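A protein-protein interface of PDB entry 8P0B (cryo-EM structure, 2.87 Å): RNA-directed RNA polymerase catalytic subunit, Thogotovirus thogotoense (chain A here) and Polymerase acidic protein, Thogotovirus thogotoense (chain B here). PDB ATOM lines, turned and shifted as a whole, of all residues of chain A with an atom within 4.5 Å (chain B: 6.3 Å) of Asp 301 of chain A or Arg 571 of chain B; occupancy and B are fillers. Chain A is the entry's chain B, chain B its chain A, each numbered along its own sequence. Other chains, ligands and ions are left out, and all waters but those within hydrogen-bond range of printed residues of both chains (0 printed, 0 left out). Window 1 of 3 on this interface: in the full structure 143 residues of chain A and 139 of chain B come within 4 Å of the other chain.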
ATOM      1  N   GLY A 300     -10.413  25.049 -29.006  1.00  0.00           N
ATOM      2  CA  GLY A 300     -10.866  23.681 -28.854  1.00  0.00           C
ATOM      3  C   GLY A 300     -11.525  23.141 -30.100  1.00  0.00           C
ATOM      4  O   GLY A 300     -11.735  23.848 -31.088  1.00  0.00           O
ATOM      5  N   ASP A 301     -11.832  21.849 -30.035  1.00  0.00           N
ATOM      6  CA  ASP A 301     -12.581  21.154 -31.066  1.00  0.00           C
ATOM      7  C   ASP A 301     -13.663  20.315 -30.404  1.00  0.00           C
ATOM      8  O   ASP A 301     -13.557  19.941 -29.233  1.00  0.00           O
ATOM      9  CB  ASP A 301     -11.678  20.256 -31.924  1.00  0.00           C
ATOM     10  CG  ASP A 301     -10.332  20.885 -32.211  1.00  0.00           C
ATOM     11  OD1 ASP A 301     -10.276  22.113 -32.430  1.00  0.00           O
ATOM     12  OD2 ASP A 301      -9.325  20.149 -32.216  1.00  0.00           O
ATOM     13  N   GLN A 302     -14.712  20.024 -31.166  1.00  0.00           N
ATOM     14  CA  GLN A 302     -15.817  19.216 -30.674  1.00  0.00           C
ATOM     15  C   GLN A 302     -15.537  17.742 -30.933  1.00  0.00           C
ATOM     16  O   GLN A 302     -15.064  17.367 -32.009  1.00  0.00           O
ATOM     17  CB  GLN A 302     -17.134  19.624 -31.340  1.00  0.00           C
ATOM     18  CG  GLN A 302     -17.279  21.115 -31.631  1.00  0.00           C
ATOM     19  CD  GLN A 302     -17.401  21.953 -30.375  1.00  0.00           C
ATOM     20  OE1 GLN A 302     -17.107  21.491 -29.275  1.00  0.00           O
ATOM     21  NE2 GLN A 302     -17.840  23.195 -30.533  1.00  0.00           N
ATOM     22  N   GLU A 303     -15.827  16.909 -29.938  1.00  0.00           N
ATOM     23  CA  GLU A 303     -15.644  15.471 -30.063  1.00  0.00           C
ATOM     24  C   GLU A 303     -16.917  14.831 -30.595  1.00  0.00           C
ATOM     25  O   GLU A 303     -18.022  15.158 -30.155  1.00  0.00           O
ATOM     26  CB  GLU A 303     -15.270  14.848 -28.716  1.00  0.00           C
ATOM     27  CG  GLU A 303     -16.427  14.723 -27.737  1.00  0.00           C
ATOM     28  CD  GLU A 303     -15.992  14.187 -26.388  1.00  0.00           C
ATOM     29  OE1 GLU A 303     -15.190  13.230 -26.359  1.00  0.00           O
ATOM     30  OE2 GLU A 303     -16.455  14.721 -25.358  1.00  0.00           O
ATOM     31  N   ASP A 422     -16.206  22.063 -36.674  1.00  0.00           N
ATOM     32  CA  ASP A 422     -15.725  21.305 -35.527  1.00  0.00           C
ATOM     33  C   ASP A 422     -14.683  22.050 -34.705  1.00  0.00           C
ATOM     34  O   ASP A 422     -14.416  21.651 -33.567  1.00  0.00           O
ATOM     35  CB  ASP A 422     -15.132  19.972 -35.994  1.00  0.00           C
ATOM     36  CG  ASP A 422     -15.204  18.899 -34.930  1.00  0.00           C
ATOM     37  OD1 ASP A 422     -15.225  19.250 -33.734  1.00  0.00           O
ATOM     38  OD2 ASP A 422     -15.238  17.703 -35.288  1.00  0.00           O
ATOM     39  N   ASP A 423     -14.089  23.110 -35.245  1.00  0.00           N
ATOM     40  CA  ASP A 423     -13.085  23.892 -34.539  1.00  0.00           C
ATOM     41  C   ASP A 423     -13.715  25.165 -33.992  1.00  0.00           C
ATOM     42  O   ASP A 423     -14.653  25.709 -34.576  1.00  0.00           O
ATOM     43  CB  ASP A 423     -11.920  24.239 -35.468  1.00  0.00           C
ATOM     44  CG  ASP A 423     -10.667  24.633 -34.713  1.00  0.00           C
ATOM     45  OD1 ASP A 423     -10.729  24.750 -33.472  1.00  0.00           O
ATOM     46  OD2 ASP A 423      -9.619  24.826 -35.363  1.00  0.00           O
ATOM     47  N   PHE A 424     -13.201  25.640 -32.860  1.00  0.00           N
ATOM     48  CA  PHE A 424     -13.745  26.861 -32.290  1.00  0.00           C
ATOM     49  C   PHE A 424     -12.697  27.542 -31.423  1.00  0.00           C
ATOM     50  O   PHE A 424     -11.814  26.892 -30.851  1.00  0.00           O
ATOM     51  CB  PHE A 424     -15.011  26.579 -31.471  1.00  0.00           C
ATOM     52  CG  PHE A 424     -14.737  26.083 -30.083  1.00  0.00           C
ATOM     53  CD1 PHE A 424     -14.586  24.732 -29.834  1.00  0.00           C
ATOM     54  CD2 PHE A 424     -14.628  26.970 -29.026  1.00  0.00           C
ATOM     55  CE1 PHE A 424     -14.332  24.276 -28.560  1.00  0.00           C
ATOM     56  CE2 PHE A 424     -14.373  26.518 -27.752  1.00  0.00           C
ATOM     57  CZ  PHE A 424     -14.224  25.170 -27.518  1.00  0.00           C
ATOM     58  N   MET A 454     -17.634  19.438 -26.555  1.00  0.00           N
ATOM     59  CA  MET A 454     -16.258  19.867 -26.742  1.00  0.00           C
ATOM     60  C   MET A 454     -15.327  18.784 -26.216  1.00  0.00           C
ATOM     61  O   MET A 454     -15.489  18.309 -25.088  1.00  0.00           O
ATOM     62  CB  MET A 454     -16.020  21.205 -26.035  1.00  0.00           C
ATOM     63  CG  MET A 454     -15.636  21.125 -24.556  1.00  0.00           C
ATOM     64  SD  MET A 454     -15.053  22.690 -23.863  1.00  0.00           S
ATOM     65  CE  MET A 454     -15.946  23.895 -24.842  1.00  0.00           C
ATOM     66  N   SER A 455     -14.367  18.376 -27.040  1.00  0.00           N
ATOM     67  CA  SER A 455     -13.426  17.345 -26.626  1.00  0.00           C
ATOM     68  C   SER A 455     -12.600  17.878 -25.462  1.00  0.00           C
ATOM     69  O   SER A 455     -11.765  18.767 -25.659  1.00  0.00           O
ATOM     70  CB  SER A 455     -12.519  16.934 -27.783  1.00  0.00           C
ATOM     71  OG  SER A 455     -12.152  15.569 -27.679  1.00  0.00           O
ATOM     72  N   SER A 457     -10.018  16.890 -23.805  1.00  0.00           N
ATOM     73  CA  SER A 457      -8.574  16.806 -23.964  1.00  0.00           C
ATOM     74  C   SER A 457      -8.054  17.723 -25.062  1.00  0.00           C
ATOM     75  O   SER A 457      -6.862  18.040 -25.070  1.00  0.00           O
ATOM     76  CB  SER A 457      -8.162  15.363 -24.257  1.00  0.00           C
ATOM     77  OG  SER A 457      -8.717  14.474 -23.305  1.00  0.00           O
ATOM     78  N   LYS A 458      -8.913  18.156 -25.983  1.00  0.00           N
ATOM     79  CA  LYS A 458      -8.510  19.031 -27.075  1.00  0.00           C
ATOM     80  C   LYS A 458      -8.875  20.489 -26.829  1.00  0.00           C
ATOM     81  O   LYS A 458      -8.719  21.313 -27.735  1.00  0.00           O
ATOM     82  CB  LYS A 458      -9.138  18.562 -28.389  1.00  0.00           C
ATOM     83  CG  LYS A 458      -8.939  17.088 -28.684  1.00  0.00           C
ATOM     84  CD  LYS A 458      -9.062  16.805 -30.168  1.00  0.00           C
ATOM     85  CE  LYS A 458      -8.849  15.335 -30.473  1.00  0.00           C
ATOM     86  NZ  LYS A 458      -8.747  15.077 -31.934  1.00  0.00           N
ATOM     87  N   CYS A 459      -9.350  20.828 -25.635  1.00  0.00           N
ATOM     88  CA  CYS A 459      -9.761  22.186 -25.300  1.00  0.00           C
ATOM     89  C   CYS A 459      -8.787  22.758 -24.281  1.00  0.00           C
ATOM     90  O   CYS A 459      -8.586  22.169 -23.213  1.00  0.00           O
ATOM     91  CB  CYS A 459     -11.187  22.205 -24.750  1.00  0.00           C
ATOM     92  SG  CYS A 459     -12.460  21.972 -26.007  1.00  0.00           S
ATOM     93  N   ILE A 460      -8.186  23.898 -24.609  1.00  0.00           N
ATOM     94  CA  ILE A 460      -7.180  24.529 -23.763  1.00  0.00           C
ATOM     95  C   ILE A 460      -7.511  26.009 -23.634  1.00  0.00           C
ATOM     96  O   ILE A 460      -7.727  26.694 -24.642  1.00  0.00           O
ATOM     97  CB  ILE A 460      -5.761  24.328 -24.329  1.00  0.00           C
ATOM     98  CG1 ILE A 460      -5.484  22.829 -24.479  1.00  0.00           C
ATOM     99  CG2 ILE A 460      -4.718  24.991 -23.433  1.00  0.00           C
ATOM    100  CD1 ILE A 460      -4.026  22.447 -24.388  1.00  0.00           C
ATOM    101  N   GLU A 469      -5.040  28.986 -31.119  1.00  0.00           N
ATOM    102  CA  GLU A 469      -5.003  28.350 -32.426  1.00  0.00           C
ATOM    103  C   GLU A 469      -6.429  28.118 -32.899  1.00  0.00           C
ATOM    104  O   GLU A 469      -7.318  27.831 -32.094  1.00  0.00           O
ATOM    105  CB  GLU A 469      -4.230  27.023 -32.385  1.00  0.00           C
ATOM    106  CG  GLU A 469      -4.908  25.914 -31.587  1.00  0.00           C
ATOM    107  CD  GLU A 469      -5.928  25.132 -32.398  1.00  0.00           C
ATOM    108  OE1 GLU A 469      -5.935  25.262 -33.641  1.00  0.00           O
ATOM    109  OE2 GLU A 469      -6.725  24.386 -31.789  1.00  0.00           O
ATOM    110  N   LEU B 566       1.684  14.695 -34.851  1.00  0.00           N
ATOM    111  CA  LEU B 566       1.928  16.105 -35.129  1.00  0.00           C
ATOM    112  C   LEU B 566       0.668  16.935 -34.924  1.00  0.00           C
ATOM    113  O   LEU B 566       0.737  18.062 -34.422  1.00  0.00           O
ATOM    114  CB  LEU B 566       2.462  16.277 -36.550  1.00  0.00           C
ATOM    115  CG  LEU B 566       3.900  15.800 -36.770  1.00  0.00           C
ATOM    116  CD1 LEU B 566       4.249  15.814 -38.247  1.00  0.00           C
ATOM    117  CD2 LEU B 566       4.880  16.650 -35.978  1.00  0.00           C
ATOM    118  N   ALA B 567      -0.493  16.398 -35.306  1.00  0.00           N
ATOM    119  CA  ALA B 567      -1.737  17.138 -35.134  1.00  0.00           C
ATOM    120  C   ALA B 567      -2.040  17.371 -33.662  1.00  0.00           C
ATOM    121  O   ALA B 567      -2.519  18.447 -33.282  1.00  0.00           O
ATOM    122  CB  ALA B 567      -2.886  16.388 -35.805  1.00  0.00           C
ATOM    123  N   ASN B 568      -1.774  16.379 -32.815  1.00  0.00           N
ATOM    124  CA  ASN B 568      -2.095  16.492 -31.401  1.00  0.00           C
ATOM    125  C   ASN B 568      -0.970  17.091 -30.568  1.00  0.00           C
ATOM    126  O   ASN B 568      -1.191  17.393 -29.391  1.00  0.00           O
ATOM    127  CB  ASN B 568      -2.467  15.116 -30.843  1.00  0.00           C
ATOM    128  CG  ASN B 568      -3.782  14.608 -31.392  1.00  0.00           C
ATOM    129  OD1 ASN B 568      -4.813  15.268 -31.272  1.00  0.00           O
ATOM    130  ND2 ASN B 568      -3.755  13.431 -32.003  1.00  0.00           N
ATOM    131  N   MET B 569       0.223  17.270 -31.136  1.00  0.00           N
ATOM    132  CA  MET B 569       1.306  17.927 -30.416  1.00  0.00           C
ATOM    133  C   MET B 569       1.254  19.444 -30.516  1.00  0.00           C
ATOM    134  O   MET B 569       1.963  20.118 -29.763  1.00  0.00           O
ATOM    135  CB  MET B 569       2.660  17.441 -30.942  1.00  0.00           C
ATOM    136  CG  MET B 569       3.127  16.118 -30.360  1.00  0.00           C
ATOM    137  SD  MET B 569       3.237  16.118 -28.562  1.00  0.00           S
ATOM    138  CE  MET B 569       4.503  17.354 -28.295  1.00  0.00           C
ATOM    139  N   ARG B 570       0.447  19.997 -31.421  1.00  0.00           N
ATOM    140  CA  ARG B 570       0.363  21.448 -31.531  1.00  0.00           C
ATOM    141  C   ARG B 570      -0.258  22.055 -30.281  1.00  0.00           C
ATOM    142  O   ARG B 570       0.139  23.144 -29.849  1.00  0.00           O
ATOM    143  CB  ARG B 570      -0.430  21.830 -32.779  1.00  0.00           C
ATOM    144  CG  ARG B 570       0.339  21.603 -34.070  1.00  0.00           C
ATOM    145  CD  ARG B 570      -0.576  21.377 -35.261  1.00  0.00           C
ATOM    146  NE  ARG B 570       0.062  20.548 -36.275  1.00  0.00           N
ATOM    147  CZ  ARG B 570      -0.583  19.908 -37.240  1.00  0.00           C
ATOM    148  NH1 ARG B 570      -1.897  19.990 -37.366  1.00  0.00           N
ATOM    149  NH2 ARG B 570       0.109  19.169 -38.101  1.00  0.00           N
ATOM    150  N   ARG B 571      -1.223  21.360 -29.677  1.00  0.00           N
ATOM    151  CA  ARG B 571      -1.809  21.838 -28.429  1.00  0.00           C
ATOM    152  C   ARG B 571      -0.748  21.961 -27.343  1.00  0.00           C
ATOM    153  O   ARG B 571      -0.674  22.975 -26.640  1.00  0.00           O
ATOM    154  CB  ARG B 571      -2.920  20.891 -27.979  1.00  0.00           C
ATOM    155  CG  ARG B 571      -4.313  21.355 -28.336  1.00  0.00           C
ATOM    156  CD  ARG B 571      -5.354  20.371 -27.843  1.00  0.00           C
ATOM    157  NE  ARG B 571      -5.182  19.046 -28.427  1.00  0.00           N
ATOM    158  CZ  ARG B 571      -5.605  18.693 -29.634  1.00  0.00           C
ATOM    159  NH1 ARG B 571      -6.234  19.547 -30.424  1.00  0.00           N
ATOM    160  NH2 ARG B 571      -5.392  17.451 -30.058  1.00  0.00           N
ATOM    161  N   LEU B 572       0.089  20.934 -27.195  1.00  0.00           N
ATOM    162  CA  LEU B 572       1.117  20.965 -26.162  1.00  0.00           C
ATOM    163  C   LEU B 572       2.214  21.966 -26.493  1.00  0.00           C
ATOM    164  O   LEU B 572       2.783  22.581 -25.587  1.00  0.00           O
ATOM    165  CB  LEU B 572       1.704  19.568 -25.967  1.00  0.00           C
ATOM    166  CG  LEU B 572       0.693  18.488 -25.577  1.00  0.00           C
ATOM    167  CD1 LEU B 572       1.375  17.142 -25.426  1.00  0.00           C
ATOM    168  CD2 LEU B 572      -0.026  18.865 -24.295  1.00  0.00           C
ATOM    169  N   HIS B 573       2.526  22.146 -27.777  1.00  0.00           N
ATOM    170  CA  HIS B 573       3.468  23.192 -28.163  1.00  0.00           C
ATOM    171  C   HIS B 573       2.942  24.566 -27.768  1.00  0.00           C
ATOM    172  O   HIS B 573       3.682  25.395 -27.224  1.00  0.00           O
ATOM    173  CB  HIS B 573       3.722  23.122 -29.669  1.00  0.00           C
ATOM    174  CG  HIS B 573       5.078  23.603 -30.082  1.00  0.00           C
ATOM    175  ND1 HIS B 573       6.243  23.045 -29.602  1.00  0.00           N
ATOM    176  CD2 HIS B 573       5.454  24.582 -30.937  1.00  0.00           C
ATOM    177  CE1 HIS B 573       7.279  23.664 -30.140  1.00  0.00           C
ATOM    178  NE2 HIS B 573       6.828  24.600 -30.954  1.00  0.00           N
ATOM    179  N   MET B 574       1.656  24.817 -28.020  1.00  0.00           N
ATOM    180  CA  MET B 574       1.048  26.078 -27.612  1.00  0.00           C
ATOM    181  C   MET B 574       1.049  26.226 -26.096  1.00  0.00           C
ATOM    182  O   MET B 574       1.276  27.322 -25.571  1.00  0.00           O
ATOM    183  CB  MET B 574      -0.377  26.164 -28.156  1.00  0.00           C
ATOM    184  CG  MET B 574      -1.226  27.233 -27.497  1.00  0.00           C
ATOM    185  SD  MET B 574      -2.726  27.597 -28.423  1.00  0.00           S
ATOM    186  CE  MET B 574      -3.561  26.015 -28.348  1.00  0.00           C
ATOM    187  N   SER B 575       0.776  25.138 -25.375  1.00  0.00           N
ATOM    188  CA  SER B 575       0.793  25.197 -23.917  1.00  0.00           C
ATOM    189  C   SER B 575       2.184  25.535 -23.397  1.00  0.00           C
ATOM    190  O   SER B 575       2.331  26.334 -22.465  1.00  0.00           O
ATOM    191  CB  SER B 575       0.312  23.870 -23.335  1.00  0.00           C
ATOM    192  OG  SER B 575      -0.923  23.481 -23.909  1.00  0.00           O
ATOM    193  N   ARG B 576       3.218  24.930 -23.984  1.00  0.00           N
ATOM    194  CA  ARG B 576       4.583  25.258 -23.588  1.00  0.00           C
ATOM    195  C   ARG B 576       4.904  26.711 -23.896  1.00  0.00           C
ATOM    196  O   ARG B 576       5.567  27.388 -23.104  1.00  0.00           O
ATOM    197  CB  ARG B 576       5.578  24.332 -24.289  1.00  0.00           C
ATOM    198  CG  ARG B 576       7.035  24.701 -24.037  1.00  0.00           C
ATOM    199  CD  ARG B 576       7.990  23.730 -24.700  1.00  0.00           C
ATOM    200  NE  ARG B 576       7.833  22.371 -24.197  1.00  0.00           N
ATOM    201  CZ  ARG B 576       8.342  21.933 -23.055  1.00  0.00           C
ATOM    202  NH1 ARG B 576       9.049  22.723 -22.264  1.00  0.00           N
ATOM    203  NH2 ARG B 576       8.139  20.669 -22.697  1.00  0.00           N
ATOM    204  N   PRO B 593      -4.617  15.853 -22.787  1.00  0.00           N
ATOM    205  CA  PRO B 593      -4.050  15.905 -24.145  1.00  0.00           C
ATOM    206  C   PRO B 593      -2.924  14.909 -24.350  1.00  0.00           C
ATOM    207  O   PRO B 593      -2.743  14.389 -25.463  1.00  0.00           O
ATOM    208  CB  PRO B 593      -3.554  17.353 -24.266  1.00  0.00           C
ATOM    209  CG  PRO B 593      -4.243  18.106 -23.174  1.00  0.00           C
ATOM    210  CD  PRO B 593      -4.469  17.131 -22.074  1.00  0.00           C
ATOM    211  N   LYS B 596      -4.132  11.886 -26.019  1.00  0.00           N
ATOM    212  CA  LYS B 596      -4.280  12.011 -27.463  1.00  0.00           C
ATOM    213  C   LYS B 596      -2.933  11.878 -28.157  1.00  0.00           C
ATOM    214  O   LYS B 596      -2.832  11.257 -29.220  1.00  0.00           O
ATOM    215  CB  LYS B 596      -4.936  13.347 -27.811  1.00  0.00           C
ATOM    216  CG  LYS B 596      -6.352  13.503 -27.279  1.00  0.00           C
ATOM    217  CD  LYS B 596      -7.338  12.612 -28.020  1.00  0.00           C
ATOM    218  CE  LYS B 596      -8.650  12.480 -27.264  1.00  0.00           C
ATOM    219  NZ  LYS B 596      -9.404  11.264 -27.669  1.00  0.00           N
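NH2 of Arg 571 of chain B is in hydrogen-bond range of OD1 of Asn 568 of chain B (2.6 Å). The backbone carbonyl oxygen (O) of Asp 301 of chain A lies within hydrogen-bond range of the backbone NH (N) of Ser 455 of chain A (2.8 Å). OG of Ser 575 of chain B sits at hydrogen-bond distance from O of Arg 571 of chain B (2.8 Å).
Printed residues of chain B within 4 Å of Asp 301 of chain A: Arg 571 (3.6 Å). Arg 571 of chain B touches just these residues of chain A: Asp 301 (3.6 Å), Ser 457 (3.9 Å) and Lys 458 (3.5 Å). Printed residues of chain A within 4 Å of Ser 575 of chain B: Ile 460. Of the printed residues of chain B, Lys 458 of chain A touches Asn 568, Arg 571 and Lys 596. Of the printed residues of chain A, Lys 596 of chain B touches Ser 457 and Lys 458. The nearest residue of chain A that does not touch Arg 571 of chain B is Ile 460 of chain A (4.1 Å).
Ser 457 of chain A touches Arg 571 of chain B. CG of Pro 593 of chain B touches O of Ser 457 of chain A, 3.2 Å away. Ser 457 of chain A touches Lys 596 of chain B. NZ of Lys 458 of chain A touches OD1 of Asn 568 of chain B, at 3.99 Å. O of Lys 458 of chain A touches CD of Arg 571 of chain B (3.5 Å). CE of Lys 458 of chain A touches CD of Lys 596 of chain B, at 3.96 Å. Ile 460 of chain A touches Ser 575 of chain B. CG of Glu 469 of chain A touches CE of Met 574 of chain B, 3.5 Å away.
Of the 14 printed residues of chain A, 5 touch a printed residue of chain B. Hydrophobic or aromatic side chains of chain A that line the printed part of chain B: Ile 460. Along chain A the printed residues that touch a printed residue of chain B span positions 301 to 469. Printed residues of chain B that touch a printed residue of chain A: Asn 568, Arg 571, Met 574, Ser 575, Pro 593 and Lys 596.
The guanidinium group (NH1) of Arg 571 of chain B lies within salt-bridge range of the side-chain carboxylate (OD2) of Asp 301 of chain A (3.6 Å).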
